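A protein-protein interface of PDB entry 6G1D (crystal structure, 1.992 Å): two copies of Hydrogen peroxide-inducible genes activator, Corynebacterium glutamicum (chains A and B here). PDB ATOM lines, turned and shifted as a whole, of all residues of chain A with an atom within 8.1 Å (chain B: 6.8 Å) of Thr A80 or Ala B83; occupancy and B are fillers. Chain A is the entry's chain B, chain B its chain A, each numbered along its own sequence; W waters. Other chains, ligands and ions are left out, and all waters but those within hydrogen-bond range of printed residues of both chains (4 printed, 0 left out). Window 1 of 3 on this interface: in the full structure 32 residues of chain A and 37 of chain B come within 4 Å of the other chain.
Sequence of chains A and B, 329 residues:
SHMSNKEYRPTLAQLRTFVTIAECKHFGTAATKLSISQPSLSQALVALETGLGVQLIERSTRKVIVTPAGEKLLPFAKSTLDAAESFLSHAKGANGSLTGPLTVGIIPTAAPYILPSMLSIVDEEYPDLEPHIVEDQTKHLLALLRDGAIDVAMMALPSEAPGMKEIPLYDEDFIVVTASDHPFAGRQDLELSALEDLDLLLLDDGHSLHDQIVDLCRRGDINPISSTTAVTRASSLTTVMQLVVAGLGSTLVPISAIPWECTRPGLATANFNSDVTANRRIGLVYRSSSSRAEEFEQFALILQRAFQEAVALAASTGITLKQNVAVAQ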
ATOM      1  N   ARG A   9     -12.638  -0.136   9.224  1.00  0.00           N
ATOM      2  CA  ARG A   9     -11.430   0.481   9.789  1.00  0.00           C
ATOM      3  C   ARG A   9     -10.672   1.112   8.639  1.00  0.00           C
ATOM      4  O   ARG A   9     -10.392   0.443   7.686  1.00  0.00           O
ATOM      5  CB  ARG A   9     -10.546  -0.552  10.486  1.00  0.00           C
ATOM      6  CG  ARG A   9     -11.220  -1.311  11.636  1.00  0.00           C
ATOM      7  CD  ARG A   9     -10.242  -1.815  12.687  1.00  0.00           C
ATOM      8  NE  ARG A   9      -9.613  -0.698  13.405  1.00  0.00           N
ATOM      9  CZ  ARG A   9     -10.034  -0.158  14.554  1.00  0.00           C
ATOM     10  NH1 ARG A   9     -11.105  -0.637  15.195  1.00  0.00           N
ATOM     11  NH2 ARG A   9      -9.368   0.885  15.068  1.00  0.00           N
ATOM     12  N   PRO A  10     -10.366   2.420   8.710  1.00  0.00           N
ATOM     13  CA  PRO A  10      -9.595   3.023   7.608  1.00  0.00           C
ATOM     14  C   PRO A  10      -8.200   2.448   7.482  1.00  0.00           C
ATOM     15  O   PRO A  10      -7.627   1.983   8.454  1.00  0.00           O
ATOM     16  CB  PRO A  10      -9.540   4.528   7.958  1.00  0.00           C
ATOM     17  CG  PRO A  10     -10.062   4.644   9.321  1.00  0.00           C
ATOM     18  CD  PRO A  10     -10.841   3.428   9.668  1.00  0.00           C
ATOM     19  N   THR A  11      -7.694   2.421   6.258  1.00  0.00           N
ATOM     20  CA  THR A  11      -6.315   1.999   6.014  1.00  0.00           C
ATOM     21  C   THR A  11      -5.433   3.237   5.954  1.00  0.00           C
ATOM     22  O   THR A  11      -5.912   4.346   5.673  1.00  0.00           O
ATOM     23  CB  THR A  11      -6.186   1.261   4.681  1.00  0.00           C
ATOM     24  OG1 THR A  11      -6.585   2.142   3.636  1.00  0.00           O
ATOM     25  CG2 THR A  11      -7.081   0.025   4.674  1.00  0.00           C
ATOM     26  N   LEU A  12      -4.143   3.047   6.173  1.00  0.00           N
ATOM     27  CA  LEU A  12      -3.215   4.147   5.983  1.00  0.00           C
ATOM     28  C   LEU A  12      -3.273   4.666   4.542  1.00  0.00           C
ATOM     29  O   LEU A  12      -3.244   5.883   4.319  1.00  0.00           O
ATOM     30  CB  LEU A  12      -1.795   3.752   6.380  1.00  0.00           C
ATOM     31  CG  LEU A  12      -1.620   3.559   7.884  1.00  0.00           C
ATOM     32  CD1 LEU A  12      -0.361   2.757   8.172  1.00  0.00           C
ATOM     33  CD2 LEU A  12      -1.586   4.895   8.601  1.00  0.00           C
ATOM     34  N   LEU A  15      -6.080   7.092   4.211  1.00  0.00           N
ATOM     35  CA  LEU A  15      -5.727   8.328   4.882  1.00  0.00           C
ATOM     36  C   LEU A  15      -4.724   9.156   4.081  1.00  0.00           C
ATOM     37  O   LEU A  15      -4.862  10.384   4.015  1.00  0.00           O
ATOM     38  CB  LEU A  15      -5.195   8.054   6.304  1.00  0.00           C
ATOM     39  CG  LEU A  15      -6.200   7.471   7.297  1.00  0.00           C
ATOM     40  CD1 LEU A  15      -5.485   7.262   8.622  1.00  0.00           C
ATOM     41  CD2 LEU A  15      -7.417   8.370   7.438  1.00  0.00           C
ATOM     42  N   VAL A  19      -5.366  13.040   2.852  1.00  0.00           N
ATOM     43  CA  VAL A  19      -4.472  14.112   3.250  1.00  0.00           C
ATOM     44  C   VAL A  19      -3.855  14.772   1.999  1.00  0.00           C
ATOM     45  O   VAL A  19      -3.790  15.992   1.901  1.00  0.00           O
ATOM     46  CB  VAL A  19      -3.394  13.570   4.229  1.00  0.00           C
ATOM     47  CG1 VAL A  19      -2.226  14.532   4.395  1.00  0.00           C
ATOM     48  CG2 VAL A  19      -4.036  13.239   5.573  1.00  0.00           C
ATOM     49  N   LEU A  73     -11.370  16.480  10.616  1.00  0.00           N
ATOM     50  CA  LEU A  73     -10.670  15.187  10.666  1.00  0.00           C
ATOM     51  C   LEU A  73      -9.233  15.208  10.125  1.00  0.00           C
ATOM     52  O   LEU A  73      -8.436  14.325  10.459  1.00  0.00           O
ATOM     53  CB  LEU A  73     -11.497  14.118   9.935  1.00  0.00           C
ATOM     54  CG  LEU A  73     -12.787  13.743  10.681  1.00  0.00           C
ATOM     55  CD1 LEU A  73     -13.698  12.929   9.786  1.00  0.00           C
ATOM     56  CD2 LEU A  73     -12.447  12.967  11.957  1.00  0.00           C
ATOM     57  N   LEU A  74      -8.898  16.199   9.312  1.00  0.00           N
ATOM     58  CA  LEU A  74      -7.551  16.293   8.714  1.00  0.00           C
ATOM     59  C   LEU A  74      -6.414  16.148   9.726  1.00  0.00           C
ATOM     60  O   LEU A  74      -5.504  15.341   9.512  1.00  0.00           O
ATOM     61  CB  LEU A  74      -7.421  17.590   7.881  1.00  0.00           C
ATOM     62  CG  LEU A  74      -6.168  17.763   7.042  1.00  0.00           C
ATOM     63  CD1 LEU A  74      -5.990  16.586   6.069  1.00  0.00           C
ATOM     64  CD2 LEU A  74      -6.252  19.103   6.270  1.00  0.00           C
ATOM     65  N   PRO A  75      -6.457  16.891  10.855  1.00  0.00           N
ATOM     66  CA  PRO A  75      -5.343  16.721  11.817  1.00  0.00           C
ATOM     67  C   PRO A  75      -5.239  15.330  12.423  1.00  0.00           C
ATOM     68  O   PRO A  75      -4.117  14.890  12.718  1.00  0.00           O
ATOM     69  CB  PRO A  75      -5.635  17.755  12.928  1.00  0.00           C
ATOM     70  CG  PRO A  75      -6.886  18.456  12.554  1.00  0.00           C
ATOM     71  CD  PRO A  75      -7.258  18.095  11.143  1.00  0.00           C
ATOM     72  N   PHE A  76      -6.367  14.630  12.578  1.00  0.00           N
ATOM     73  CA  PHE A  76      -6.290  13.262  13.090  1.00  0.00           C
ATOM     74  C   PHE A  76      -5.688  12.305  12.039  1.00  0.00           C
ATOM     75  O   PHE A  76      -4.933  11.405  12.388  1.00  0.00           O
ATOM     76  CB  PHE A  76      -7.669  12.789  13.553  1.00  0.00           C
ATOM     77  CG  PHE A  76      -8.220  13.562  14.692  1.00  0.00           C
ATOM     78  CD1 PHE A  76      -7.856  13.234  15.977  1.00  0.00           C
ATOM     79  CD2 PHE A  76      -9.154  14.566  14.494  1.00  0.00           C
ATOM     80  CE1 PHE A  76      -8.411  13.928  17.088  1.00  0.00           C
ATOM     81  CE2 PHE A  76      -9.713  15.255  15.583  1.00  0.00           C
ATOM     82  CZ  PHE A  76      -9.327  14.942  16.867  1.00  0.00           C
ATOM     83  N   ALA A  77      -6.021  12.528  10.771  1.00  0.00           N
ATOM     84  CA  ALA A  77      -5.440  11.741   9.669  1.00  0.00           C
ATOM     85  C   ALA A  77      -3.930  11.971   9.617  1.00  0.00           C
ATOM     86  O   ALA A  77      -3.154  11.013   9.628  1.00  0.00           O
ATOM     87  CB  ALA A  77      -6.097  12.117   8.363  1.00  0.00           C
ATOM     88  N   LYS A  78      -3.519  13.244   9.640  1.00  0.00           N
ATOM     89  CA  LYS A  78      -2.086  13.571   9.686  1.00  0.00           C
ATOM     90  C   LYS A  78      -1.345  12.952  10.862  1.00  0.00           C
ATOM     91  O   LYS A  78      -0.251  12.433  10.679  1.00  0.00           O
ATOM     92  CB  LYS A  78      -1.853  15.073   9.670  1.00  0.00           C
ATOM     93  CG  LYS A  78      -2.044  15.650   8.314  1.00  0.00           C
ATOM     94  CD  LYS A  78      -2.203  17.155   8.531  1.00  0.00           C
ATOM     95  CE  LYS A  78      -2.088  17.926   7.257  1.00  0.00           C
ATOM     96  NZ  LYS A  78      -0.668  18.204   6.901  1.00  0.00           N
ATOM     97  N   SER A  79      -1.919  12.999  12.061  1.00  0.00           N
ATOM     98  CA  SER A  79      -1.263  12.375  13.232  1.00  0.00           C
ATOM     99  C   SER A  79      -1.030  10.890  13.019  1.00  0.00           C
ATOM    100  O   SER A  79       0.004  10.357  13.449  1.00  0.00           O
ATOM    101  CB  SER A  79      -2.089  12.514  14.522  1.00  0.00           C
ATOM    102  OG  SER A  79      -2.493  13.835  14.698  1.00  0.00           O
ATOM    103  N   THR A  80      -1.991  10.225  12.377  1.00  0.00           N
ATOM    104  CA  THR A  80      -1.875   8.784  12.172  1.00  0.00           C
ATOM    105  C   THR A  80      -0.717   8.476  11.220  1.00  0.00           C
ATOM    106  O   THR A  80       0.104   7.583  11.505  1.00  0.00           O
ATOM    107  CB  THR A  80      -3.198   8.184  11.643  1.00  0.00           C
ATOM    108  OG1 THR A  80      -4.298   8.624  12.465  1.00  0.00           O
ATOM    109  CG2 THR A  80      -3.124   6.661  11.633  1.00  0.00           C
ATOM    110  N   LEU A  81      -0.659   9.240  10.120  1.00  0.00           N
ATOM    111  CA  LEU A  81       0.384   9.075   9.114  1.00  0.00           C
ATOM    112  C   LEU A  81       1.750   9.385   9.710  1.00  0.00           C
ATOM    113  O   LEU A  81       2.717   8.684   9.415  1.00  0.00           O
ATOM    114  CB  LEU A  81       0.126   9.953   7.892  1.00  0.00           C
ATOM    115  CG  LEU A  81      -1.167   9.611   7.133  1.00  0.00           C
ATOM    116  CD1 LEU A  81      -1.468  10.586   5.995  1.00  0.00           C
ATOM    117  CD2 LEU A  81      -1.117   8.194   6.604  1.00  0.00           C
ATOM    118  N   ASP A  82       1.822  10.416  10.561  1.00  0.00           N
ATOM    119  CA  ASP A  82       3.077  10.789  11.229  1.00  0.00           C
ATOM    120  C   ASP A  82       3.517   9.704  12.208  1.00  0.00           C
ATOM    121  O   ASP A  82       4.697   9.359  12.268  1.00  0.00           O
ATOM    122  CB  ASP A  82       2.953  12.134  11.961  1.00  0.00           C
ATOM    123  CG  ASP A  82       2.709  13.333  11.009  1.00  0.00           C
ATOM    124  OD1 ASP A  82       2.885  13.207   9.773  1.00  0.00           O
ATOM    125  OD2 ASP A  82       2.328  14.419  11.517  1.00  0.00           O
ATOM    126  N   ALA A  83       2.580   9.160  12.982  1.00  0.00           N
ATOM    127  CA  ALA A  83       2.935   8.031  13.857  1.00  0.00           C
ATOM    128  C   ALA A  83       3.429   6.800  13.041  1.00  0.00           C
ATOM    129  O   ALA A  83       4.380   6.131  13.438  1.00  0.00           O
ATOM    130  CB  ALA A  83       1.767   7.650  14.745  1.00  0.00           C
ATOM    131  N   ALA A  84       2.797   6.524  11.901  1.00  0.00           N
ATOM    132  CA  ALA A  84       3.210   5.382  11.074  1.00  0.00           C
ATOM    133  C   ALA A  84       4.604   5.596  10.463  1.00  0.00           C
ATOM    134  O   ALA A  84       5.412   4.684  10.457  1.00  0.00           O
ATOM    135  CB  ALA A  84       2.200   5.119   9.978  1.00  0.00           C
ATOM    136  N   GLU A  85       4.872   6.806   9.965  1.00  0.00           N
ATOM    137  CA  GLU A  85       6.209   7.169   9.470  1.00  0.00           C
ATOM    138  C   GLU A  85       7.259   7.020  10.566  1.00  0.00           C
ATOM    139  O   GLU A  85       8.337   6.489  10.325  1.00  0.00           O
ATOM    140  CB  GLU A  85       6.239   8.611   8.912  1.00  0.00           C
ATOM    141  CG  GLU A  85       6.103   8.746   7.415  1.00  0.00           C
ATOM    142  CD  GLU A  85       7.178   7.971   6.660  1.00  0.00           C
ATOM    143  OE1 GLU A  85       8.391   8.265   6.801  1.00  0.00           O
ATOM    144  OE2 GLU A  85       6.798   7.048   5.918  1.00  0.00           O
ATOM    145  N   SER A  86       6.939   7.466  11.778  1.00  0.00           N
ATOM    146  CA  SER A  86       7.872   7.313  12.879  1.00  0.00           C
ATOM    147  C   SER A  86       8.162   5.845  13.217  1.00  0.00           C
ATOM    148  O   SER A  86       9.312   5.485  13.531  1.00  0.00           O
ATOM    149  CB  SER A  86       7.378   8.063  14.118  1.00  0.00           C
ATOM    150  OG  SER A  86       8.290   7.871  15.193  1.00  0.00           O
ATOM    151  N   PHE A  87       7.138   4.979  13.146  1.00  0.00           N
ATOM    152  CA  PHE A  87       7.354   3.538  13.349  1.00  0.00           C
ATOM    153  C   PHE A  87       8.336   3.007  12.304  1.00  0.00           C
ATOM    154  O   PHE A  87       9.296   2.314  12.632  1.00  0.00           O
ATOM    155  CB  PHE A  87       6.031   2.758  13.280  1.00  0.00           C
ATOM    156  CG  PHE A  87       6.202   1.278  13.332  1.00  0.00           C
ATOM    157  CD1 PHE A  87       6.255   0.618  14.541  1.00  0.00           C
ATOM    158  CD2 PHE A  87       6.329   0.534  12.148  1.00  0.00           C
ATOM    159  CE1 PHE A  87       6.383  -0.765  14.589  1.00  0.00           C
ATOM    160  CE2 PHE A  87       6.481  -0.841  12.191  1.00  0.00           C
ATOM    161  CZ  PHE A  87       6.514  -1.498  13.410  1.00  0.00           C
ATOM    162  N   LEU B  12      -2.060  -0.796   9.076  1.00  0.00           N
ATOM    163  CA  LEU B  12      -2.624  -0.807  10.417  1.00  0.00           C
ATOM    164  C   LEU B  12      -2.965  -2.241  10.872  1.00  0.00           C
ATOM    165  O   LEU B  12      -2.703  -2.585  12.017  1.00  0.00           O
ATOM    166  CB  LEU B  12      -3.846   0.113  10.519  1.00  0.00           C
ATOM    167  CG  LEU B  12      -3.450   1.589  10.454  1.00  0.00           C
ATOM    168  CD1 LEU B  12      -4.628   2.480  10.105  1.00  0.00           C
ATOM    169  CD2 LEU B  12      -2.819   2.034  11.763  1.00  0.00           C
ATOM    170  N   LYS B  78       1.988   1.262  18.971  1.00  0.00           N
ATOM    171  CA  LYS B  78       0.876   1.664  19.815  1.00  0.00           C
ATOM    172  C   LYS B  78       0.410   3.077  19.497  1.00  0.00           C
ATOM    173  O   LYS B  78      -0.779   3.321  19.400  1.00  0.00           O
ATOM    174  CB  LYS B  78       1.304   1.616  21.277  1.00  0.00           C
ATOM    175  CG  LYS B  78       0.580   0.601  22.129  1.00  0.00           C
ATOM    176  CD  LYS B  78      -0.860   1.019  22.379  1.00  0.00           C
ATOM    177  CE  LYS B  78      -1.450   0.280  23.566  1.00  0.00           C
ATOM    178  NZ  LYS B  78      -2.934   0.366  23.622  1.00  0.00           N
ATOM    179  N   SER B  79       1.345   4.003  19.317  1.00  0.00           N
ATOM    180  CA  SER B  79       0.976   5.386  18.972  1.00  0.00           C
ATOM    181  C   SER B  79       0.200   5.456  17.693  1.00  0.00           C
ATOM    182  O   SER B  79      -0.750   6.263  17.583  1.00  0.00           O
ATOM    183  CB  SER B  79       2.206   6.303  18.813  1.00  0.00           C
ATOM    184  OG  SER B  79       3.078   6.158  19.906  1.00  0.00           O
ATOM    185  N   THR B  80       0.596   4.624  16.714  1.00  0.00           N
ATOM    186  CA  THR B  80      -0.052   4.659  15.420  1.00  0.00           C
ATOM    187  C   THR B  80      -1.507   4.202  15.535  1.00  0.00           C
ATOM    188  O   THR B  80      -2.429   4.841  14.997  1.00  0.00           O
ATOM    189  CB  THR B  80       0.717   3.816  14.384  1.00  0.00           C
ATOM    190  OG1 THR B  80       2.123   4.126  14.410  1.00  0.00           O
ATOM    191  CG2 THR B  80       0.155   4.068  12.982  1.00  0.00           C
ATOM    192  N   LEU B  81      -1.695   3.099  16.253  1.00  0.00           N
ATOM    193  CA  LEU B  81      -3.026   2.539  16.455  1.00  0.00           C
ATOM    194  C   LEU B  81      -3.902   3.453  17.263  1.00  0.00           C
ATOM    195  O   LEU B  81      -5.072   3.574  16.950  1.00  0.00           O
ATOM    196  CB  LEU B  81      -2.919   1.162  17.144  1.00  0.00           C
ATOM    197  CG  LEU B  81      -2.202   0.101  16.301  1.00  0.00           C
ATOM    198  CD1 LEU B  81      -2.169  -1.113  17.174  1.00  0.00           C
ATOM    199  CD2 LEU B  81      -2.956  -0.089  14.994  1.00  0.00           C
ATOM    200  N   ASP B  82      -3.326   4.133  18.252  1.00  0.00           N
ATOM    201  CA  ASP B  82      -4.076   5.123  19.069  1.00  0.00           C
ATOM    202  C   ASP B  82      -4.480   6.324  18.211  1.00  0.00           C
ATOM    203  O   ASP B  82      -5.617   6.784  18.296  1.00  0.00           O
ATOM    204  CB  ASP B  82      -3.268   5.585  20.278  1.00  0.00           C
ATOM    205  CG  ASP B  82      -2.991   4.443  21.303  1.00  0.00           C
ATOM    206  OD1 ASP B  82      -3.617   3.362  21.239  1.00  0.00           O
ATOM    207  OD2 ASP B  82      -2.124   4.619  22.197  1.00  0.00           O
ATOM    208  N   ALA B  83      -3.567   6.818  17.374  1.00  0.00           N
ATOM    209  CA  ALA B  83      -3.957   7.877  16.444  1.00  0.00           C
ATOM    210  C   ALA B  83      -5.089   7.436  15.471  1.00  0.00           C
ATOM    211  O   ALA B  83      -6.021   8.201  15.187  1.00  0.00           O
ATOM    212  CB  ALA B  83      -2.748   8.393  15.682  1.00  0.00           C
ATOM    213  N   ALA B  84      -5.018   6.201  14.983  1.00  0.00           N
ATOM    214  CA  ALA B  84      -6.046   5.712  14.049  1.00  0.00           C
ATOM    215  C   ALA B  84      -7.393   5.540  14.724  1.00  0.00           C
ATOM    216  O   ALA B  84      -8.417   5.910  14.153  1.00  0.00           O
ATOM    217  CB  ALA B  84      -5.616   4.389  13.412  1.00  0.00           C
ATOM    218  N   GLU B  85      -7.398   4.996  15.948  1.00  0.00           N
ATOM    219  CA  GLU B  85      -8.635   4.885  16.753  1.00  0.00           C
ATOM    220  C   GLU B  85      -9.229   6.258  17.000  1.00  0.00           C
ATOM    221  O   GLU B  85     -10.443   6.445  16.874  1.00  0.00           O
ATOM    222  CB  GLU B  85      -8.361   4.179  18.093  1.00  0.00           C
ATOM    223  CG  GLU B  85      -9.658   3.835  18.898  1.00  0.00           C
ATOM    224  CD  GLU B  85     -10.934   3.351  18.088  1.00  0.00           C
ATOM    225  OE1 GLU B  85     -11.938   4.118  18.037  1.00  0.00           O
ATOM    226  OE2 GLU B  85     -10.996   2.227  17.496  1.00  0.00           O
ATOM    227  N   SER B  86      -8.391   7.230  17.334  1.00  0.00           N
ATOM    228  CA  SER B  86      -8.896   8.595  17.548  1.00  0.00           C
ATOM    229  C   SER B  86      -9.510   9.204  16.285  1.00  0.00           C
ATOM    230  O   SER B  86     -10.529   9.892  16.372  1.00  0.00           O
ATOM    231  CB  SER B  86      -7.785   9.496  18.090  1.00  0.00           C
ATOM    232  OG  SER B  86      -8.281  10.790  18.290  1.00  0.00           O
ATOM    233  N   PHE B  87      -8.925   8.934  15.109  1.00  0.00           N
ATOM    234  CA  PHE B  87      -9.524   9.396  13.842  1.00  0.00           C
ATOM    235  C   PHE B  87     -10.911   8.805  13.677  1.00  0.00           C
ATOM    236  O   PHE B  87     -11.887   9.524  13.381  1.00  0.00           O
ATOM    237  CB  PHE B  87      -8.648   9.019  12.634  1.00  0.00           C
ATOM    238  CG  PHE B  87      -9.267   9.350  11.320  1.00  0.00           C
ATOM    239  CD1 PHE B  87      -9.078  10.599  10.755  1.00  0.00           C
ATOM    240  CD2 PHE B  87     -10.046   8.415  10.635  1.00  0.00           C
ATOM    241  CE1 PHE B  87      -9.615  10.905   9.514  1.00  0.00           C
ATOM    242  CE2 PHE B  87     -10.587   8.724   9.398  1.00  0.00           C
ATOM    243  CZ  PHE B  87     -10.374   9.973   8.829  1.00  0.00           C
ATOM    244  N   LEU B  88     -11.001   7.491  13.876  1.00  0.00           N
ATOM    245  CA  LEU B  88     -12.257   6.795  13.661  1.00  0.00           C
ATOM    246  C   LEU B  88     -13.344   7.263  14.643  1.00  0.00           C
ATOM    247  O   LEU B  88     -14.483   7.507  14.239  1.00  0.00           O
ATOM    248  CB  LEU B  88     -12.030   5.269  13.781  1.00  0.00           C
ATOM    249  CG  LEU B  88     -13.240   4.381  13.495  1.00  0.00           C
ATOM    250  CD1 LEU B  88     -13.875   4.699  12.142  1.00  0.00           C
ATOM    251  CD2 LEU B  88     -12.804   2.919  13.615  1.00  0.00           C
HETATM  252  O   HOH W   1      -9.328   3.258  13.274  1.00  0.00           O
HETATM  253  O   HOH W   2      -6.420   1.477  15.936  1.00  0.00           O
HETATM  254  O   HOH W   3      -5.561  10.686  15.273  1.00  0.00           O
HETATM  255  O   HOH W   4      -3.328   0.272   6.668  1.00  0.00           O
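The side-chain hydroxyl (OG1) of Thr B80 sits at hydrogen-bond distance from the backbone carbonyl oxygen (O) of Ala A83 (3.2 Å). The guanidinium group (NH2) of Arg A9 lies within salt-bridge range of the side-chain carboxylate (OE2) of Glu B85 (3.2 Å). The side-chain hydroxyl (OG1) of Thr A80 is in hydrogen-bond range of the backbone carbonyl oxygen (O) of Ala B83 (3.2 Å).
OG1 of Thr A80 is in hydrogen-bond range of O of Phe A76 (2.9 Å).
Pro A10 touches Leu B12. Phe B87 touches Pro A10. Leu B12 touches Leu A12 (CG to CG, 3.7 Å). Leu A15 touches Phe B87. O of Leu A73 touches CE1 of Phe B87, at 3.7 Å. Phe A76 touches Ser B86. Phe B87 touches Phe A76. O of Thr A80 touches CG2 of Thr B80 (3.8 Å). Thr A80 touches Ala B84 (OG1 to N, 3.6 Å). Ala A83 touches Ser B79.
Of chain B, only Thr B80 (3.8 Å), Ala B83 (3.2 Å) and Ala B84 (3.6 Å) come within 4 Å of Thr A80. Ala B83 touches one residue of chain A. Of chain A, only Thr A80 comes within 4 Å of Ala B84. Of the printed residues of chain A, Ser B79 touches Ala A83. Printed residues of chain B within 4 Å of Arg A9: Glu B85. Printed residues of chain A within 4 Å of Glu B85: Arg A9 (3.2 Å). Leu B81 touches none of the printed residues of chain A. Pro A75 touches none of the printed residues of chain B. The nearest residue of chain A that does not touch Ala B83 is Ser A79 (4.03 Å). The nearest printed residue of chain B that does not touch Arg A9 is Leu B88 (4.2 Å).
Hydrophobic or aromatic side chains of chain B that line the printed part of chain A: Leu B12, Ala B83, Ala B84 and Phe B87. Of the 21 printed residues of chain A, 10 touch a printed residue of chain B. Printed residues of chain A that touch a printed residue of chain B: Arg A9, Pro A10, Leu A12, Leu A15, Leu A73, Phe A76, Ala A77, Thr A80, Ala A83 and Ala A84. Hydrophobic or aromatic side chains of chain A within 4 Å of the printed part of chain B: Pro A10, Leu A12, Leu A15, Leu A73, Phe A76, Ala A77, Ala A83 and Ala A84. Among the printed residues, 15 pairs touch across the chains. Among the printed residues, Asp or Glu carboxylates within 4 Å of a Lys or Arg side-chain nitrogen of the other chain: Arg A9 with Glu B85 (3.2 Å).
Leu A12 touches its own counterpart, Leu B12. Thr B80 touches its own counterpart, Thr A80. Thr A80 touches Ala B84, and with the chains exchanged Ala A84 touches Thr B80. Ala A83 touches Ser B79, but with the chains exchanged Ser A79 does not touch Ala B83 (4.03 Å). 11 positions are printed for both chains. Of the 15 pairs that touch across the chains among the printed residues, 6 have their exchanged pair printed and touching as well.
Water W3 bridges the backbone carbonyl oxygen (O) of Ala B83 (2.5 Å) and the backbone carbonyl oxygen (O) of Phe A76 (3.0 Å). Water W2 bridges the backbone carbonyl oxygen of Leu B81 and the guanidinium group of Arg A9. Water W4 bridges N of Leu B12 (2.9 Å) and N of Leu A12 (2.9 Å). Water W1 bridges the backbone carbonyl oxygen of Ala B84 (2.9 Å) and the guanidinium group of Arg A9 (3.0 Å).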
